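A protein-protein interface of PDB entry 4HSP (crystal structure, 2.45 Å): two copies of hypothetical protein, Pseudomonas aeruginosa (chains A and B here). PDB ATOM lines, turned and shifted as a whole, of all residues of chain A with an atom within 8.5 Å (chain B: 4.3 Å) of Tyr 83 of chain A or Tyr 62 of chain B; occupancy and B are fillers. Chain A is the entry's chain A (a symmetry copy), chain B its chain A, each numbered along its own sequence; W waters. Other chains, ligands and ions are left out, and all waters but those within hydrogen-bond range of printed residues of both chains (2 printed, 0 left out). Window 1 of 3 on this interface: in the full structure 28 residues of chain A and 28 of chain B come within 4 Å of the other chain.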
ATOM      1  N   PRO A  22     -30.377 -13.559 -12.706  1.00  0.00           N
ATOM      2  CA  PRO A  22     -30.697 -13.231 -11.309  1.00  0.00           C
ATOM      3  C   PRO A  22     -31.173 -11.782 -11.139  1.00  0.00           C
ATOM      4  O   PRO A  22     -31.795 -11.490 -10.121  1.00  0.00           O
ATOM      5  CB  PRO A  22     -29.364 -13.476 -10.581  1.00  0.00           C
ATOM      6  CG  PRO A  22     -28.597 -14.372 -11.467  1.00  0.00           C
ATOM      7  CD  PRO A  22     -28.943 -13.865 -12.845  1.00  0.00           C
ATOM      8  N   LEU A  23     -30.865 -10.880 -12.115  1.00  0.00           N
ATOM      9  CA  LEU A  23     -31.298  -9.484 -12.152  1.00  0.00           C
ATOM     10  C   LEU A  23     -32.187  -9.272 -13.358  1.00  0.00           C
ATOM     11  O   LEU A  23     -31.662  -8.929 -14.422  1.00  0.00           O
ATOM     12  CB  LEU A  23     -30.109  -8.520 -12.221  1.00  0.00           C
ATOM     13  CG  LEU A  23     -29.424  -8.162 -10.931  1.00  0.00           C
ATOM     14  CD1 LEU A  23     -28.055  -7.612 -11.225  1.00  0.00           C
ATOM     15  CD2 LEU A  23     -30.277  -7.170 -10.113  1.00  0.00           C
ATOM     16  N   GLY A  61     -24.496 -21.057  -0.612  1.00  0.00           N
ATOM     17  CA  GLY A  61     -25.604 -20.156  -0.904  1.00  0.00           C
ATOM     18  C   GLY A  61     -25.878 -19.087   0.130  1.00  0.00           C
ATOM     19  O   GLY A  61     -25.120 -18.922   1.081  1.00  0.00           O
ATOM     20  N   TYR A  62     -26.956 -18.323  -0.093  1.00  0.00           N
ATOM     21  CA  TYR A  62     -27.387 -17.248   0.784  1.00  0.00           C
ATOM     22  C   TYR A  62     -28.639 -17.672   1.529  1.00  0.00           C
ATOM     23  O   TYR A  62     -29.421 -18.477   1.027  1.00  0.00           O
ATOM     24  CB  TYR A  62     -27.614 -15.955  -0.049  1.00  0.00           C
ATOM     25  CG  TYR A  62     -26.301 -15.294  -0.405  1.00  0.00           C
ATOM     26  CD1 TYR A  62     -25.687 -14.407   0.476  1.00  0.00           C
ATOM     27  CD2 TYR A  62     -25.612 -15.641  -1.571  1.00  0.00           C
ATOM     28  CE1 TYR A  62     -24.467 -13.809   0.165  1.00  0.00           C
ATOM     29  CE2 TYR A  62     -24.399 -15.032  -1.902  1.00  0.00           C
ATOM     30  CZ  TYR A  62     -23.830 -14.119  -1.025  1.00  0.00           C
ATOM     31  OH  TYR A  62     -22.616 -13.538  -1.284  1.00  0.00           O
ATOM     32  N   ILE A  63     -28.801 -17.176   2.758  1.00  0.00           N
ATOM     33  CA  ILE A  63     -29.914 -17.565   3.627  1.00  0.00           C
ATOM     34  C   ILE A  63     -31.041 -16.506   3.662  1.00  0.00           C
ATOM     35  O   ILE A  63     -30.772 -15.331   3.918  1.00  0.00           O
ATOM     36  CB  ILE A  63     -29.364 -17.840   5.029  1.00  0.00           C
ATOM     37  CG1 ILE A  63     -28.436 -19.089   5.006  1.00  0.00           C
ATOM     38  CG2 ILE A  63     -30.501 -17.945   6.071  1.00  0.00           C
ATOM     39  CD1 ILE A  63     -27.744 -19.412   6.406  1.00  0.00           C
ATOM     40  N   VAL A  64     -32.286 -16.960   3.316  1.00  0.00           N
ATOM     41  CA  VAL A  64     -33.549 -16.239   3.374  1.00  0.00           C
ATOM     42  C   VAL A  64     -34.268 -16.797   4.607  1.00  0.00           C
ATOM     43  O   VAL A  64     -34.843 -17.883   4.526  1.00  0.00           O
ATOM     44  CB  VAL A  64     -34.399 -16.330   2.079  1.00  0.00           C
ATOM     45  CG1 VAL A  64     -35.668 -15.490   2.208  1.00  0.00           C
ATOM     46  CG2 VAL A  64     -33.600 -15.884   0.859  1.00  0.00           C
ATOM     47  N   VAL A  80     -30.593 -20.213  -1.267  1.00  0.00           N
ATOM     48  CA  VAL A  80     -30.702 -19.688  -2.627  1.00  0.00           C
ATOM     49  C   VAL A  80     -29.275 -19.412  -3.170  1.00  0.00           C
ATOM     50  O   VAL A  80     -28.338 -19.218  -2.375  1.00  0.00           O
ATOM     51  CB  VAL A  80     -31.598 -18.408  -2.623  1.00  0.00           C
ATOM     52  CG1 VAL A  80     -33.065 -18.755  -2.321  1.00  0.00           C
ATOM     53  CG2 VAL A  80     -31.072 -17.393  -1.615  1.00  0.00           C
ATOM     54  N   PRO A  81     -29.100 -19.349  -4.506  1.00  0.00           N
ATOM     55  CA  PRO A  81     -27.745 -19.152  -5.054  1.00  0.00           C
ATOM     56  C   PRO A  81     -27.280 -17.687  -5.087  1.00  0.00           C
ATOM     57  O   PRO A  81     -26.151 -17.413  -5.493  1.00  0.00           O
ATOM     58  CB  PRO A  81     -27.849 -19.720  -6.490  1.00  0.00           C
ATOM     59  CG  PRO A  81     -29.278 -20.123  -6.687  1.00  0.00           C
ATOM     60  CD  PRO A  81     -30.088 -19.548  -5.592  1.00  0.00           C
ATOM     61  N   TYR A  82     -28.147 -16.746  -4.739  1.00  0.00           N
ATOM     62  CA  TYR A  82     -27.756 -15.354  -4.785  1.00  0.00           C
ATOM     63  C   TYR A  82     -28.443 -14.575  -3.697  1.00  0.00           C
ATOM     64  O   TYR A  82     -29.560 -14.910  -3.273  1.00  0.00           O
ATOM     65  CB  TYR A  82     -27.981 -14.703  -6.174  1.00  0.00           C
ATOM     66  CG  TYR A  82     -29.325 -14.961  -6.812  1.00  0.00           C
ATOM     67  CD1 TYR A  82     -29.516 -16.037  -7.665  1.00  0.00           C
ATOM     68  CD2 TYR A  82     -30.387 -14.081  -6.629  1.00  0.00           C
ATOM     69  CE1 TYR A  82     -30.743 -16.275  -8.268  1.00  0.00           C
ATOM     70  CE2 TYR A  82     -31.625 -14.306  -7.236  1.00  0.00           C
ATOM     71  CZ  TYR A  82     -31.794 -15.404  -8.062  1.00  0.00           C
ATOM     72  OH  TYR A  82     -32.998 -15.659  -8.679  1.00  0.00           O
ATOM     73  N   TYR A  83     -27.724 -13.557  -3.205  1.00  0.00           N
ATOM     74  CA  TYR A  83     -28.212 -12.677  -2.176  1.00  0.00           C
ATOM     75  C   TYR A  83     -29.367 -11.860  -2.731  1.00  0.00           C
ATOM     76  O   TYR A  83     -29.336 -11.447  -3.887  1.00  0.00           O
ATOM     77  CB  TYR A  83     -27.066 -11.785  -1.676  1.00  0.00           C
ATOM     78  CG  TYR A  83     -27.500 -10.711  -0.707  1.00  0.00           C
ATOM     79  CD1 TYR A  83     -27.583 -10.967   0.657  1.00  0.00           C
ATOM     80  CD2 TYR A  83     -27.867  -9.443  -1.158  1.00  0.00           C
ATOM     81  CE1 TYR A  83     -28.023  -9.990   1.553  1.00  0.00           C
ATOM     82  CE2 TYR A  83     -28.319  -8.465  -0.277  1.00  0.00           C
ATOM     83  CZ  TYR A  83     -28.390  -8.737   1.079  1.00  0.00           C
ATOM     84  OH  TYR A  83     -28.798  -7.748   1.950  1.00  0.00           O
ATOM     85  N   GLY A  84     -30.363 -11.635  -1.894  1.00  0.00           N
ATOM     86  CA  GLY A  84     -31.521 -10.821  -2.241  1.00  0.00           C
ATOM     87  C   GLY A  84     -32.699 -11.570  -2.825  1.00  0.00           C
ATOM     88  O   GLY A  84     -33.786 -10.995  -2.933  1.00  0.00           O
ATOM     89  N   ALA A  85     -32.493 -12.846  -3.218  1.00  0.00           N
ATOM     90  CA  ALA A  85     -33.527 -13.707  -3.789  1.00  0.00           C
ATOM     91  C   ALA A  85     -34.730 -13.708  -2.895  1.00  0.00           C
ATOM     92  O   ALA A  85     -34.579 -13.915  -1.688  1.00  0.00           O
ATOM     93  CB  ALA A  85     -33.003 -15.117  -3.957  1.00  0.00           C
ATOM     94  N   CYS A  86     -35.909 -13.366  -3.483  1.00  0.00           N
ATOM     95  CA  CYS A  86     -37.263 -13.266  -2.914  1.00  0.00           C
ATOM     96  C   CYS A  86     -37.529 -11.912  -2.311  1.00  0.00           C
ATOM     97  O   CYS A  86     -38.692 -11.574  -2.125  1.00  0.00           O
ATOM     98  CB  CYS A  86     -37.557 -14.373  -1.902  1.00  0.00           C
ATOM     99  SG  CYS A  86     -37.202 -16.045  -2.504  1.00  0.00           S
ATOM    100  N   ILE A  87     -36.482 -11.138  -1.992  1.00  0.00           N
ATOM    101  CA  ILE A  87     -36.607  -9.844  -1.314  1.00  0.00           C
ATOM    102  C   ILE A  87     -36.366  -8.670  -2.256  1.00  0.00           C
ATOM    103  O   ILE A  87     -37.252  -7.833  -2.418  1.00  0.00           O
ATOM    104  CB  ILE A  87     -35.624  -9.810  -0.102  1.00  0.00           C
ATOM    105  CG1 ILE A  87     -35.984 -10.897   0.941  1.00  0.00           C
ATOM    106  CG2 ILE A  87     -35.514  -8.418   0.536  1.00  0.00           C
ATOM    107  CD1 ILE A  87     -34.964 -11.982   1.010  1.00  0.00           C
ATOM    108  N   HIS A  88     -35.167  -8.579  -2.828  1.00  0.00           N
ATOM    109  CA  HIS A  88     -34.772  -7.478  -3.702  1.00  0.00           C
ATOM    110  C   HIS A  88     -35.017  -7.780  -5.179  1.00  0.00           C
ATOM    111  O   HIS A  88     -35.218  -6.857  -5.963  1.00  0.00           O
ATOM    112  CB  HIS A  88     -33.303  -7.105  -3.456  1.00  0.00           C
ATOM    113  CG  HIS A  88     -33.059  -6.554  -2.078  1.00  0.00           C
ATOM    114  ND1 HIS A  88     -32.013  -7.014  -1.288  1.00  0.00           N
ATOM    115  CD2 HIS A  88     -33.739  -5.605  -1.391  1.00  0.00           C
ATOM    116  CE1 HIS A  88     -32.091  -6.332  -0.161  1.00  0.00           C
ATOM    117  NE2 HIS A  88     -33.124  -5.481  -0.175  1.00  0.00           N
ATOM    118  N   VAL A  89     -35.034  -9.056  -5.543  1.00  0.00           N
ATOM    119  CA  VAL A  89     -35.307  -9.547  -6.893  1.00  0.00           C
ATOM    120  C   VAL A  89     -36.317 -10.687  -6.778  1.00  0.00           C
ATOM    121  O   VAL A  89     -36.410 -11.271  -5.694  1.00  0.00           O
ATOM    122  CB  VAL A  89     -34.005 -10.027  -7.623  1.00  0.00           C
ATOM    123  CG1 VAL A  89     -33.103  -8.852  -8.031  1.00  0.00           C
ATOM    124  CG2 VAL A  89     -33.243 -11.059  -6.794  1.00  0.00           C
ATOM    125  N   PRO A  90     -37.006 -11.098  -7.871  1.00  0.00           N
ATOM    126  CA  PRO A  90     -37.939 -12.243  -7.772  1.00  0.00           C
ATOM    127  C   PRO A  90     -37.304 -13.553  -7.290  1.00  0.00           C
ATOM    128  O   PRO A  90     -36.113 -13.773  -7.500  1.00  0.00           O
ATOM    129  CB  PRO A  90     -38.436 -12.421  -9.214  1.00  0.00           C
ATOM    130  CG  PRO A  90     -38.304 -11.085  -9.821  1.00  0.00           C
ATOM    131  CD  PRO A  90     -37.064 -10.481  -9.212  1.00  0.00           C
ATOM    132  N   PRO A  92     -35.860 -17.384  -7.151  1.00  0.00           N
ATOM    133  CA  PRO A  92     -35.328 -18.263  -8.220  1.00  0.00           C
ATOM    134  C   PRO A  92     -36.326 -19.375  -8.587  1.00  0.00           C
ATOM    135  O   PRO A  92     -37.289 -19.566  -7.831  1.00  0.00           O
ATOM    136  CB  PRO A  92     -34.068 -18.888  -7.576  1.00  0.00           C
ATOM    137  CG  PRO A  92     -33.826 -18.155  -6.330  1.00  0.00           C
ATOM    138  CD  PRO A  92     -35.144 -17.604  -5.877  1.00  0.00           C
ATOM    139  N   GLU A 110     -25.365 -12.084  10.901  1.00  0.00           N
ATOM    140  CA  GLU A 110     -24.388 -12.544   9.928  1.00  0.00           C
ATOM    141  C   GLU A 110     -24.982 -13.229   8.647  1.00  0.00           C
ATOM    142  O   GLU A 110     -24.309 -14.069   8.056  1.00  0.00           O
ATOM    143  CB  GLU A 110     -23.335 -13.440  10.623  1.00  0.00           C
ATOM    144  CG  GLU A 110     -23.838 -14.686  11.340  1.00  0.00           C
ATOM    145  CD  GLU A 110     -22.763 -15.635  11.849  1.00  0.00           C
ATOM    146  OE1 GLU A 110     -21.563 -15.395  11.572  1.00  0.00           O
ATOM    147  OE2 GLU A 110     -23.126 -16.643  12.500  1.00  0.00           O
ATOM    148  N   LEU A 111     -26.150 -12.772   8.143  1.00  0.00           N
ATOM    149  CA  LEU A 111     -26.775 -13.334   6.939  1.00  0.00           C
ATOM    150  C   LEU A 111     -26.462 -12.546   5.658  1.00  0.00           C
ATOM    151  O   LEU A 111     -27.096 -12.774   4.625  1.00  0.00           O
ATOM    152  CB  LEU A 111     -28.302 -13.457   7.096  1.00  0.00           C
ATOM    153  CG  LEU A 111     -28.846 -14.365   8.219  1.00  0.00           C
ATOM    154  CD1 LEU A 111     -30.368 -14.429   8.166  1.00  0.00           C
ATOM    155  CD2 LEU A 111     -28.269 -15.769   8.150  1.00  0.00           C
ATOM    156  N   TYR A 112     -25.469 -11.657   5.712  1.00  0.00           N
ATOM    157  CA  TYR A 112     -24.995 -10.804   4.607  1.00  0.00           C
ATOM    158  C   TYR A 112     -23.974 -11.580   3.776  1.00  0.00           C
ATOM    159  O   TYR A 112     -23.620 -11.180   2.672  1.00  0.00           O
ATOM    160  CB  TYR A 112     -24.355  -9.503   5.188  1.00  0.00           C
ATOM    161  CG  TYR A 112     -23.158  -9.774   6.091  1.00  0.00           C
ATOM    162  CD1 TYR A 112     -23.332 -10.156   7.421  1.00  0.00           C
ATOM    163  CD2 TYR A 112     -21.856  -9.748   5.589  1.00  0.00           C
ATOM    164  CE1 TYR A 112     -22.245 -10.508   8.225  1.00  0.00           C
ATOM    165  CE2 TYR A 112     -20.760 -10.082   6.391  1.00  0.00           C
ATOM    166  CZ  TYR A 112     -20.960 -10.466   7.708  1.00  0.00           C
ATOM    167  OH  TYR A 112     -19.894 -10.782   8.520  1.00  0.00           O
ATOM    168  N   GLN A 113     -23.461 -12.672   4.344  1.00  0.00           N
ATOM    169  CA  GLN A 113     -22.421 -13.504   3.735  1.00  0.00           C
ATOM    170  C   GLN A 113     -22.994 -14.825   3.252  1.00  0.00           C
ATOM    171  O   GLN A 113     -24.059 -15.240   3.752  1.00  0.00           O
ATOM    172  CB  GLN A 113     -21.291 -13.750   4.763  1.00  0.00           C
ATOM    173  CG  GLN A 113     -21.645 -14.717   5.880  1.00  0.00           C
ATOM    174  CD  GLN A 113     -20.772 -14.533   7.077  1.00  0.00           C
ATOM    175  OE1 GLN A 113     -19.552 -14.699   7.036  1.00  0.00           O
ATOM    176  NE2 GLN A 113     -21.392 -14.188   8.173  1.00  0.00           N
ATOM    177  N   PRO A 114     -22.301 -15.515   2.298  1.00  0.00           N
ATOM    178  CA  PRO A 114     -22.773 -16.838   1.903  1.00  0.00           C
ATOM    179  C   PRO A 114     -22.328 -17.868   2.933  1.00  0.00           C
ATOM    180  O   PRO A 114     -21.427 -17.609   3.746  1.00  0.00           O
ATOM    181  CB  PRO A 114     -22.125 -17.056   0.533  1.00  0.00           C
ATOM    182  CG  PRO A 114     -20.956 -16.143   0.492  1.00  0.00           C
ATOM    183  CD  PRO A 114     -21.000 -15.210   1.659  1.00  0.00           C
ATOM    184  N   GLY B  61     -27.349  -3.719 -11.058  1.00  0.00           N
ATOM    185  CA  GLY B  61     -26.253  -4.375 -10.356  1.00  0.00           C
ATOM    186  C   GLY B  61     -26.051  -3.964  -8.914  1.00  0.00           C
ATOM    187  O   GLY B  61     -26.853  -3.225  -8.352  1.00  0.00           O
ATOM    188  N   TYR B  62     -24.984  -4.495  -8.301  1.00  0.00           N
ATOM    189  CA  TYR B  62     -24.619  -4.221  -6.922  1.00  0.00           C
ATOM    190  C   TYR B  62     -23.389  -3.332  -6.889  1.00  0.00           C
ATOM    191  O   TYR B  62     -22.567  -3.372  -7.801  1.00  0.00           O
ATOM    192  CB  TYR B  62     -24.389  -5.561  -6.168  1.00  0.00           C
ATOM    193  CG  TYR B  62     -25.702  -6.221  -5.810  1.00  0.00           C
ATOM    194  CD1 TYR B  62     -26.377  -5.883  -4.639  1.00  0.00           C
ATOM    195  CD2 TYR B  62     -26.332  -7.101  -6.696  1.00  0.00           C
ATOM    196  CE1 TYR B  62     -27.597  -6.471  -4.313  1.00  0.00           C
ATOM    197  CE2 TYR B  62     -27.544  -7.712  -6.369  1.00  0.00           C
ATOM    198  CZ  TYR B  62     -28.174  -7.387  -5.174  1.00  0.00           C
ATOM    199  OH  TYR B  62     -29.391  -7.922  -4.838  1.00  0.00           O
ATOM    200  N   ILE B  63     -23.294  -2.481  -5.865  1.00  0.00           N
ATOM    201  CA  ILE B  63     -22.209  -1.504  -5.748  1.00  0.00           C
ATOM    202  C   ILE B  63     -21.112  -1.946  -4.752  1.00  0.00           C
ATOM    203  O   ILE B  63     -21.422  -2.284  -3.608  1.00  0.00           O
ATOM    204  CB  ILE B  63     -22.811  -0.153  -5.352  1.00  0.00           C
ATOM    205  CG1 ILE B  63     -23.705   0.395  -6.501  1.00  0.00           C
ATOM    206  CG2 ILE B  63     -21.718   0.842  -4.902  1.00  0.00           C
ATOM    207  CD1 ILE B  63     -24.448   1.762  -6.154  1.00  0.00           C
ATOM    208  N   VAL B  64     -19.843  -2.003  -5.261  1.00  0.00           N
ATOM    209  CA  VAL B  64     -18.602  -2.262  -4.545  1.00  0.00           C
ATOM    210  C   VAL B  64     -17.922  -0.893  -4.422  1.00  0.00           C
ATOM    211  O   VAL B  64     -17.317  -0.436  -5.392  1.00  0.00           O
ATOM    212  CB  VAL B  64     -17.695  -3.337  -5.200  1.00  0.00           C
ATOM    213  CG1 VAL B  64     -16.455  -3.589  -4.346  1.00  0.00           C
ATOM    214  CG2 VAL B  64     -18.452  -4.642  -5.419  1.00  0.00           C
ATOM    215  N   LEU B  78     -17.329  -0.079  -8.264  1.00  0.00           N
ATOM    216  CA  LEU B  78     -17.491  -1.129  -9.271  1.00  0.00           C
ATOM    217  C   LEU B  78     -18.950  -1.571  -9.262  1.00  0.00           C
ATOM    218  O   LEU B  78     -19.511  -1.806  -8.188  1.00  0.00           O
ATOM    219  CB  LEU B  78     -16.571  -2.338  -9.025  1.00  0.00           C
ATOM    220  CG  LEU B  78     -15.052  -2.115  -8.888  1.00  0.00           C
ATOM    221  CD1 LEU B  78     -14.347  -3.432  -8.516  1.00  0.00           C
ATOM    222  CD2 LEU B  78     -14.420  -1.494 -10.175  1.00  0.00           C
ATOM    223  N   LEU B  79     -19.573  -1.634 -10.450  1.00  0.00           N
ATOM    224  CA  LEU B  79     -20.901  -2.188 -10.676  1.00  0.00           C
ATOM    225  C   LEU B  79     -20.670  -3.613 -11.115  1.00  0.00           C
ATOM    226  O   LEU B  79     -19.897  -3.875 -12.043  1.00  0.00           O
ATOM    227  CB  LEU B  79     -21.716  -1.387 -11.716  1.00  0.00           C
ATOM    228  CG  LEU B  79     -23.186  -1.783 -11.860  1.00  0.00           C
ATOM    229  CD1 LEU B  79     -23.981  -1.461 -10.540  1.00  0.00           C
ATOM    230  CD2 LEU B  79     -23.800  -1.094 -13.051  1.00  0.00           C
ATOM    231  N   VAL B  80     -21.253  -4.540 -10.363  1.00  0.00           N
ATOM    232  CA  VAL B  80     -21.100  -5.983 -10.539  1.00  0.00           C
ATOM    233  C   VAL B  80     -22.508  -6.628 -10.614  1.00  0.00           C
ATOM    234  O   VAL B  80     -23.483  -6.044 -10.107  1.00  0.00           O
ATOM    235  CB  VAL B  80     -20.237  -6.562  -9.372  1.00  0.00           C
ATOM    236  CG1 VAL B  80     -18.777  -6.095  -9.472  1.00  0.00           C
ATOM    237  CG2 VAL B  80     -20.832  -6.170  -8.025  1.00  0.00           C
ATOM    238  N   TYR B  82     -23.635  -9.301  -9.058  1.00  0.00           N
ATOM    239  CA  TYR B  82     -24.060 -10.011  -7.870  1.00  0.00           C
ATOM    240  C   TYR B  82     -23.441  -9.405  -6.641  1.00  0.00           C
ATOM    241  O   TYR B  82     -22.334  -8.845  -6.688  1.00  0.00           O
ATOM    242  CB  TYR B  82     -23.792 -11.537  -7.945  1.00  0.00           C
ATOM    243  CG  TYR B  82     -22.416 -11.941  -8.416  1.00  0.00           C
ATOM    244  CD1 TYR B  82     -22.161 -12.178  -9.757  1.00  0.00           C
ATOM    245  CD2 TYR B  82     -21.386 -12.170  -7.509  1.00  0.00           C
ATOM    246  CE1 TYR B  82     -20.903 -12.564 -10.200  1.00  0.00           C
ATOM    247  CE2 TYR B  82     -20.118 -12.566  -7.940  1.00  0.00           C
ATOM    248  CZ  TYR B  82     -19.885 -12.769  -9.290  1.00  0.00           C
ATOM    249  OH  TYR B  82     -18.650 -13.160  -9.754  1.00  0.00           O
ATOM    250  N   TYR B  83     -24.206  -9.473  -5.544  1.00  0.00           N
ATOM    251  CA  TYR B  83     -23.785  -8.971  -4.262  1.00  0.00           C
ATOM    252  C   TYR B  83     -22.629  -9.818  -3.755  1.00  0.00           C
ATOM    253  O   TYR B  83     -22.620 -11.032  -3.939  1.00  0.00           O
ATOM    254  CB  TYR B  83     -24.974  -8.984  -3.289  1.00  0.00           C
ATOM    255  CG  TYR B  83     -24.610  -8.628  -1.868  1.00  0.00           C
ATOM    256  CD1 TYR B  83     -24.579  -7.304  -1.445  1.00  0.00           C
ATOM    257  CD2 TYR B  83     -24.257  -9.617  -0.949  1.00  0.00           C
ATOM    258  CE1 TYR B  83     -24.203  -6.968  -0.142  1.00  0.00           C
ATOM    259  CE2 TYR B  83     -23.868  -9.294   0.348  1.00  0.00           C
ATOM    260  CZ  TYR B  83     -23.848  -7.969   0.752  1.00  0.00           C
ATOM    261  OH  TYR B  83     -23.504  -7.660   2.052  1.00  0.00           O
ATOM    262  N   TYR B 112     -26.889  -2.582   0.246  1.00  0.00           N
ATOM    263  CA  TYR B 112     -27.337  -3.971   0.454  1.00  0.00           C
ATOM    264  C   TYR B 112     -28.301  -4.361  -0.665  1.00  0.00           C
ATOM    265  O   TYR B 112     -28.618  -5.531  -0.850  1.00  0.00           O
ATOM    266  CB  TYR B 112     -28.035  -4.093   1.847  1.00  0.00           C
ATOM    267  CG  TYR B 112     -29.263  -3.200   1.984  1.00  0.00           C
ATOM    268  CD1 TYR B 112     -29.136  -1.844   2.284  1.00  0.00           C
ATOM    269  CD2 TYR B 112     -30.542  -3.688   1.714  1.00  0.00           C
ATOM    270  CE1 TYR B 112     -30.247  -0.998   2.307  1.00  0.00           C
ATOM    271  CE2 TYR B 112     -31.662  -2.852   1.752  1.00  0.00           C
ATOM    272  CZ  TYR B 112     -31.509  -1.506   2.045  1.00  0.00           C
ATOM    273  OH  TYR B 112     -32.601  -0.668   2.105  1.00  0.00           O
ATOM    274  N   GLN B 113     -28.810  -3.357  -1.380  1.00  0.00           N
ATOM    275  CA  GLN B 113     -29.802  -3.525  -2.445  1.00  0.00           C
ATOM    276  C   GLN B 113     -29.174  -3.310  -3.811  1.00  0.00           C
ATOM    277  O   GLN B 113     -28.122  -2.646  -3.894  1.00  0.00           O
ATOM    278  CB  GLN B 113     -30.968  -2.533  -2.223  1.00  0.00           C
ATOM    279  CG  GLN B 113     -30.637  -1.083  -2.531  1.00  0.00           C
ATOM    280  CD  GLN B 113     -31.565  -0.139  -1.841  1.00  0.00           C
ATOM    281  OE1 GLN B 113     -32.778  -0.127  -2.060  1.00  0.00           O
ATOM    282  NE2 GLN B 113     -31.002   0.679  -0.993  1.00  0.00           N
ATOM    283  N   PRO B 114     -29.808  -3.840  -4.899  1.00  0.00           N
ATOM    284  CA  PRO B 114     -29.285  -3.548  -6.230  1.00  0.00           C
ATOM    285  C   PRO B 114     -29.748  -2.166  -6.669  1.00  0.00           C
ATOM    286  O   PRO B 114     -30.690  -1.596  -6.095  1.00  0.00           O
ATOM    287  CB  PRO B 114     -29.869  -4.668  -7.097  1.00  0.00           C
ATOM    288  CG  PRO B 114     -31.058  -5.168  -6.363  1.00  0.00           C
ATOM    289  CD  PRO B 114     -31.088  -4.581  -4.988  1.00  0.00           C
HETATM  290  O   HOH W   1     -25.228 -12.902  -4.470  1.00  0.00           O
HETATM  291  O   HOH W   2     -26.662 -10.961  -5.672  1.00  0.00           O
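Hydrophobic or aromatic side chains of chain B within 4 Å of the printed part of chain A: Tyr 62, Tyr 83, Tyr 112 and Pro 114. Hydrophobic or aromatic side chains of chain A that line the printed part of chain B: Leu 23, Tyr 62, Tyr 83, His 88 and Tyr 112.
Gly 61 of chain B touches Leu 23 of chain A (CA to CD1, 3.8 Å). CB of Pro 114 of chain B touches CD2 of Leu 23 of chain A, at 3.9 Å. Tyr 62 of chain A touches Tyr 83 of chain B (OH to O, 3.7 Å). O of Tyr 83 of chain A touches OH of Tyr 62 of chain B (3.7 Å). CG of Tyr 83 of chain A touches CD2 of Tyr 83 of chain B (3.4 Å). Tyr 83 of chain A touches Tyr 112 of chain B. His 88 of chain A touches Tyr 112 of chain B (NE2 to CE2, 3.6 Å). Pro 114 of chain B touches His 88 of chain A. Tyr 112 of chain A touches Tyr 83 of chain B.
Tyr 62 of chain A touches Tyr 83 of chain B, and with the chains exchanged Tyr 83 of chain A touches Tyr 62 of chain B. Tyr 83 of chain A touches its own counterpart, Tyr 83 of chain B. Tyr 83 of chain A touches Tyr 112 of chain B, and with the chains exchanged Tyr 112 of chain A touches Tyr 83 of chain B. Positions printed for both chains: 61, 62, 63, 64, 80, 82, 83, 112, 113 and 114.
Water W2 bridges N of Tyr 83 of chain B and O of Tyr 83 of chain A. Water W1 bridges N of Tyr 83 of chain A (2.9 Å) and O of Tyr 83 of chain B (3.3 Å).
Of chain B, only Tyr 62 (3.7 Å), Tyr 83 (3.4 Å) and Tyr 112 (3.0 Å) come within 4 Å of Tyr 83 of chain A. Of chain A, only Tyr 83 (3.7 Å) comes within 4 Å of Tyr 62 of chain B. Printed residues of chain A within 4 Å of Gly 61 of chain B: Leu 23. Printed residues of chain B within 4 Å of Tyr 62 of chain A: Tyr 83. Of the printed residues of chain A, Tyr 112 of chain B touches Tyr 83 (3.0 Å) and His 88 (3.6 Å). Of the printed residues of chain B, Tyr 112 of chain A touches Tyr 83 (3.0 Å). Ile 63 of chain A touches none of the printed residues of chain B. Val 80 of chain B touches none of the printed residues of chain A. The nearest printed residue of chain A that does not touch Tyr 83 of chain B is Gln 113 of chain A (5.2 Å).
O of Val 80 of chain A lies within hydrogen-bond range of N of Tyr 62 of chain A (2.8 Å). The backbone NH (N) of Tyr 62 of chain B lies within hydrogen-bond range of the backbone carbonyl oxygen (O) of Val 80 of chain B (2.8 Å).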
